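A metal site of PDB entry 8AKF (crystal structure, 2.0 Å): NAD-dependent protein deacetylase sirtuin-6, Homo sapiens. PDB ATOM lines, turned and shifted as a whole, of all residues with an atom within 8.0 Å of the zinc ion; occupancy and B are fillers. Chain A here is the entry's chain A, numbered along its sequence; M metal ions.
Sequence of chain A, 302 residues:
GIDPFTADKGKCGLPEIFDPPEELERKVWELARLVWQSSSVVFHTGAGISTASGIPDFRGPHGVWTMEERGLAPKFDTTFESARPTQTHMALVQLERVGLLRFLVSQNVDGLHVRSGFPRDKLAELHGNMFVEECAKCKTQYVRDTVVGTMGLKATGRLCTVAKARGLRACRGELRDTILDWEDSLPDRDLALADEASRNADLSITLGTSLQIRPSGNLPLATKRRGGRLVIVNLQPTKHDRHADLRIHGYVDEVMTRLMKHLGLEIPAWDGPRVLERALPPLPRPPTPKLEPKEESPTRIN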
ATOM      1  N   GLU A 134      -0.753 -23.985   4.600  1.00  0.00           N
ATOM      2  CA  GLU A 134       0.396 -24.430   5.430  1.00  0.00           C
ATOM      3  C   GLU A 134       0.019 -24.241   6.897  1.00  0.00           C
ATOM      4  O   GLU A 134      -0.625 -23.226   7.193  1.00  0.00           O
ATOM      5  CB  GLU A 134       1.625 -23.593   5.077  1.00  0.00           C
ATOM      6  CG  GLU A 134       2.928 -24.208   5.553  1.00  0.00           C
ATOM      7  CD  GLU A 134       4.139 -23.512   4.961  1.00  0.00           C
ATOM      8  OE1 GLU A 134       4.300 -23.568   3.730  1.00  0.00           O
ATOM      9  OE2 GLU A 134       4.884 -22.874   5.728  1.00  0.00           O
ATOM     10  N   CYS A 135       0.468 -25.134   7.772  1.00  0.00           N
ATOM     11  CA  CYS A 135       0.277 -25.013   9.242  1.00  0.00           C
ATOM     12  C   CYS A 135       1.385 -24.112   9.774  1.00  0.00           C
ATOM     13  O   CYS A 135       2.559 -24.354   9.454  1.00  0.00           O
ATOM     14  CB  CYS A 135       0.300 -26.386   9.911  1.00  0.00           C
ATOM     15  SG  CYS A 135       0.174 -26.360  11.730  1.00  0.00           S
ATOM     16  N   ALA A 136       1.027 -23.083  10.537  1.00  0.00           N
ATOM     17  CA  ALA A 136       2.013 -22.184  11.182  1.00  0.00           C
ATOM     18  C   ALA A 136       2.869 -22.970  12.170  1.00  0.00           C
ATOM     19  O   ALA A 136       4.098 -22.787  12.160  1.00  0.00           O
ATOM     20  CB  ALA A 136       1.281 -21.084  11.876  1.00  0.00           C
ATOM     21  N   LYS A 137       2.234 -23.806  13.006  1.00  0.00           N
ATOM     22  CA  LYS A 137       2.924 -24.551  14.090  1.00  0.00           C
ATOM     23  C   LYS A 137       3.878 -25.607  13.506  1.00  0.00           C
ATOM     24  O   LYS A 137       5.064 -25.589  13.879  1.00  0.00           O
ATOM     25  CB  LYS A 137       1.920 -25.237  15.015  1.00  0.00           C
ATOM     26  CG  LYS A 137       1.148 -24.308  15.946  1.00  0.00           C
ATOM     27  CD  LYS A 137       0.361 -25.075  16.989  1.00  0.00           C
ATOM     28  CE  LYS A 137      -0.334 -24.187  17.989  1.00  0.00           C
ATOM     29  NZ  LYS A 137      -1.164 -24.975  18.935  1.00  0.00           N
ATOM     30  N   CYS A 138       3.395 -26.496  12.629  1.00  0.00           N
ATOM     31  CA  CYS A 138       4.203 -27.663  12.182  1.00  0.00           C
ATOM     32  C   CYS A 138       4.667 -27.521  10.728  1.00  0.00           C
ATOM     33  O   CYS A 138       5.473 -28.350  10.314  1.00  0.00           O
ATOM     34  CB  CYS A 138       3.438 -28.958  12.401  1.00  0.00           C
ATOM     35  SG  CYS A 138       2.048 -29.181  11.252  1.00  0.00           S
ATOM     36  N   LYS A 139       4.160 -26.518  10.001  1.00  0.00           N
ATOM     37  CA  LYS A 139       4.560 -26.193   8.604  1.00  0.00           C
ATOM     38  C   LYS A 139       4.008 -27.247   7.632  1.00  0.00           C
ATOM     39  O   LYS A 139       4.426 -27.211   6.470  1.00  0.00           O
ATOM     40  CB  LYS A 139       6.078 -26.018   8.513  1.00  0.00           C
ATOM     41  CG  LYS A 139       6.673 -25.013   9.490  1.00  0.00           C
ATOM     42  CD  LYS A 139       6.205 -23.603   9.279  1.00  0.00           C
ATOM     43  CE  LYS A 139       6.919 -22.600  10.178  1.00  0.00           C
ATOM     44  NZ  LYS A 139       6.486 -21.212   9.904  1.00  0.00           N
ATOM     45  N   THR A 140       3.124 -28.141   8.081  1.00  0.00           N
ATOM     46  CA  THR A 140       2.515 -29.182   7.209  1.00  0.00           C
ATOM     47  C   THR A 140       1.726 -28.470   6.102  1.00  0.00           C
ATOM     48  O   THR A 140       1.029 -27.476   6.412  1.00  0.00           O
ATOM     49  CB  THR A 140       1.578 -30.140   7.954  1.00  0.00           C
ATOM     50  OG1 THR A 140       2.322 -30.944   8.873  1.00  0.00           O
ATOM     51  CG2 THR A 140       0.819 -31.061   7.019  1.00  0.00           C
ATOM     52  N   GLN A 141       1.809 -28.987   4.865  1.00  0.00           N
ATOM     53  CA  GLN A 141       1.100 -28.412   3.692  1.00  0.00           C
ATOM     54  C   GLN A 141      -0.059 -29.322   3.288  1.00  0.00           C
ATOM     55  O   GLN A 141       0.088 -30.553   3.404  1.00  0.00           O
ATOM     56  CB  GLN A 141       2.046 -28.187   2.523  1.00  0.00           C
ATOM     57  CG  GLN A 141       2.985 -27.016   2.763  1.00  0.00           C
ATOM     58  CD  GLN A 141       3.945 -26.834   1.613  1.00  0.00           C
ATOM     59  OE1 GLN A 141       4.376 -27.788   0.981  1.00  0.00           O
ATOM     60  NE2 GLN A 141       4.309 -25.586   1.354  1.00  0.00           N
ATOM     61  N   TYR A 142      -1.177 -28.724   2.869  1.00  0.00           N
ATOM     62  CA  TYR A 142      -2.407 -29.400   2.363  1.00  0.00           C
ATOM     63  C   TYR A 142      -2.718 -28.881   0.958  1.00  0.00           C
ATOM     64  O   TYR A 142      -2.844 -27.667   0.777  1.00  0.00           O
ATOM     65  CB  TYR A 142      -3.603 -29.099   3.263  1.00  0.00           C
ATOM     66  CG  TYR A 142      -3.442 -29.453   4.717  1.00  0.00           C
ATOM     67  CD1 TYR A 142      -2.704 -28.659   5.573  1.00  0.00           C
ATOM     68  CD2 TYR A 142      -4.060 -30.587   5.240  1.00  0.00           C
ATOM     69  CE1 TYR A 142      -2.545 -28.979   6.908  1.00  0.00           C
ATOM     70  CE2 TYR A 142      -3.940 -30.910   6.587  1.00  0.00           C
ATOM     71  CZ  TYR A 142      -3.174 -30.106   7.413  1.00  0.00           C
ATOM     72  OH  TYR A 142      -3.062 -30.414   8.738  1.00  0.00           O
ATOM     73  N   LEU A 159      -7.896 -25.617  10.523  1.00  0.00           N
ATOM     74  CA  LEU A 159      -6.885 -25.974  11.558  1.00  0.00           C
ATOM     75  C   LEU A 159      -6.239 -27.299  11.169  1.00  0.00           C
ATOM     76  O   LEU A 159      -6.892 -28.157  10.550  1.00  0.00           O
ATOM     77  CB  LEU A 159      -7.540 -26.056  12.942  1.00  0.00           C
ATOM     78  CG  LEU A 159      -8.044 -24.744  13.547  1.00  0.00           C
ATOM     79  CD1 LEU A 159      -8.794 -24.998  14.849  1.00  0.00           C
ATOM     80  CD2 LEU A 159      -6.882 -23.779  13.783  1.00  0.00           C
ATOM     81  N   CYS A 160      -4.985 -27.473  11.568  1.00  0.00           N
ATOM     82  CA  CYS A 160      -4.157 -28.633  11.171  1.00  0.00           C
ATOM     83  C   CYS A 160      -4.760 -29.941  11.714  1.00  0.00           C
ATOM     84  O   CYS A 160      -5.454 -29.855  12.728  1.00  0.00           O
ATOM     85  CB  CYS A 160      -2.755 -28.406  11.670  1.00  0.00           C
ATOM     86  SG  CYS A 160      -1.660 -29.697  11.056  1.00  0.00           S
ATOM     87  N   THR A 161      -4.533 -31.072  11.027  1.00  0.00           N
ATOM     88  CA  THR A 161      -5.068 -32.421  11.403  1.00  0.00           C
ATOM     89  C   THR A 161      -3.934 -33.441  11.569  1.00  0.00           C
ATOM     90  O   THR A 161      -4.245 -34.647  11.536  1.00  0.00           O
ATOM     91  CB  THR A 161      -6.061 -32.991  10.378  1.00  0.00           C
ATOM     92  OG1 THR A 161      -5.367 -33.433   9.207  1.00  0.00           O
ATOM     93  CG2 THR A 161      -7.135 -32.013   9.967  1.00  0.00           C
ATOM     94  N   VAL A 162      -2.680 -33.007  11.718  1.00  0.00           N
ATOM     95  CA  VAL A 162      -1.539 -33.949  11.925  1.00  0.00           C
ATOM     96  C   VAL A 162      -1.790 -34.698  13.233  1.00  0.00           C
ATOM     97  O   VAL A 162      -1.832 -34.038  14.294  1.00  0.00           O
ATOM     98  CB  VAL A 162      -0.182 -33.218  11.944  1.00  0.00           C
ATOM     99  CG1 VAL A 162       0.915 -34.074  12.561  1.00  0.00           C
ATOM    100  CG2 VAL A 162       0.228 -32.752  10.549  1.00  0.00           C
ATOM    101  N   ALA A 163      -1.985 -36.020  13.152  1.00  0.00           N
ATOM    102  CA  ALA A 163      -2.356 -36.935  14.259  1.00  0.00           C
ATOM    103  C   ALA A 163      -2.237 -36.232  15.610  1.00  0.00           C
ATOM    104  O   ALA A 163      -1.095 -36.129  16.118  1.00  0.00           O
ATOM    105  CB  ALA A 163      -1.486 -38.178  14.191  1.00  0.00           C
ATOM    106  N   CYS A 171      -2.538 -31.495  16.372  1.00  0.00           N
ATOM    107  CA  CYS A 171      -1.823 -30.217  16.151  1.00  0.00           C
ATOM    108  C   CYS A 171      -2.768 -29.033  16.347  1.00  0.00           C
ATOM    109  O   CYS A 171      -2.397 -28.111  17.091  1.00  0.00           O
ATOM    110  CB  CYS A 171      -1.220 -30.160  14.751  1.00  0.00           C
ATOM    111  SG  CYS A 171      -0.017 -28.823  14.565  1.00  0.00           S
ATOM    112  N   ARG A 172      -3.930 -29.053  15.689  1.00  0.00           N
ATOM    113  CA  ARG A 172      -4.969 -27.979  15.765  1.00  0.00           C
ATOM    114  C   ARG A 172      -4.312 -26.615  15.506  1.00  0.00           C
ATOM    115  O   ARG A 172      -4.881 -25.589  15.925  1.00  0.00           O
ATOM    116  CB  ARG A 172      -5.710 -28.038  17.106  1.00  0.00           C
ATOM    117  CG  ARG A 172      -6.908 -28.978  17.121  1.00  0.00           C
ATOM    118  CD  ARG A 172      -7.619 -29.038  18.459  1.00  0.00           C
ATOM    119  NE  ARG A 172      -7.971 -27.709  18.934  1.00  0.00           N
ATOM    120  CZ  ARG A 172      -9.089 -27.052  18.652  1.00  0.00           C
ATOM    121  NH1 ARG A 172     -10.032 -27.604  17.906  1.00  0.00           N
ATOM    122  NH2 ARG A 172      -9.269 -25.831  19.134  1.00  0.00           N
ATOM    123  N   GLY A 173      -3.177 -26.600  14.804  1.00  0.00           N
ATOM    124  CA  GLY A 173      -2.473 -25.369  14.440  1.00  0.00           C
ATOM    125  C   GLY A 173      -3.212 -24.613  13.363  1.00  0.00           C
ATOM    126  O   GLY A 173      -3.983 -25.235  12.606  1.00  0.00           O
ATOM    127  N   GLU A 174      -2.978 -23.303  13.289  1.00  0.00           N
ATOM    128  CA  GLU A 174      -3.584 -22.368  12.311  1.00  0.00           C
ATOM    129  C   GLU A 174      -3.102 -22.677  10.894  1.00  0.00           C
ATOM    130  O   GLU A 174      -1.897 -22.607  10.649  1.00  0.00           O
ATOM    131  CB  GLU A 174      -3.198 -20.922  12.655  1.00  0.00           C
ATOM    132  CG  GLU A 174      -4.073 -19.883  12.003  1.00  0.00           C
ATOM    133  CD  GLU A 174      -4.125 -18.612  12.837  1.00  0.00           C
ATOM    134  OE1 GLU A 174      -4.441 -18.732  14.048  1.00  0.00           O
ATOM    135  OE2 GLU A 174      -3.826 -17.523  12.290  1.00  0.00           O
ATOM    136  N   LEU A 175      -4.038 -23.002   9.997  1.00  0.00           N
ATOM    137  CA  LEU A 175      -3.789 -23.125   8.539  1.00  0.00           C
ATOM    138  C   LEU A 175      -3.868 -21.727   7.925  1.00  0.00           C
ATOM    139  O   LEU A 175      -4.814 -21.001   8.267  1.00  0.00           O
ATOM    140  CB  LEU A 175      -4.828 -24.067   7.912  1.00  0.00           C
ATOM    141  CG  LEU A 175      -4.692 -25.542   8.259  1.00  0.00           C
ATOM    142  CD1 LEU A 175      -5.358 -26.401   7.192  1.00  0.00           C
ATOM    143  CD2 LEU A 175      -3.240 -25.963   8.439  1.00  0.00           C
HETATM  144 ZN    ZN M   1       0.116 -28.764  12.207  1.00  0.00          ZN
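The zinc ion is bound by the side-chain sulfur (SG) of Cys 138 (2.2 Å), the side-chain sulfur (SG) of Cys 160 (2.3 Å), the side-chain sulfur (SG) of Cys 171 (2.4 Å) and the side-chain sulfur (SG) of Cys 135 (2.5 Å). The zinc ion has four donor atoms within binding distance.
Of the 19 residues printed, 4 come within 4 Å of the zinc ion. The nearest printed residue that does not touch the zinc ion is Val 162 (4.3 Å).
SG of Cys 160 sits close to N of Val 162. The backbone carbonyl oxygen of Thr 140 lies within hydrogen-bond range of the backbone NH of Cys 135, at 2.8 Å. The side-chain sulfur (SG) of Cys 138 sits close to the side-chain hydroxyl (OG1) of Thr 140, at 3.0 Å. The backbone NH (N) of Cys 171 is in hydrogen-bond range of the backbone carbonyl oxygen (O) of Val 162 (3.4 Å). O of Cys 160 lies within hydrogen-bond range of N of Arg 172 (3.4 Å). N of Cys 160 lies within hydrogen-bond range of O of Gly 173, 2.7 Å away. The side-chain sulfur (SG) of Cys 160 lies close to the side-chain hydroxyl (OH) of Tyr 142, 2.8 Å away. N of Lys 137 sits close to SG of Cys 135, at 3.5 Å.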
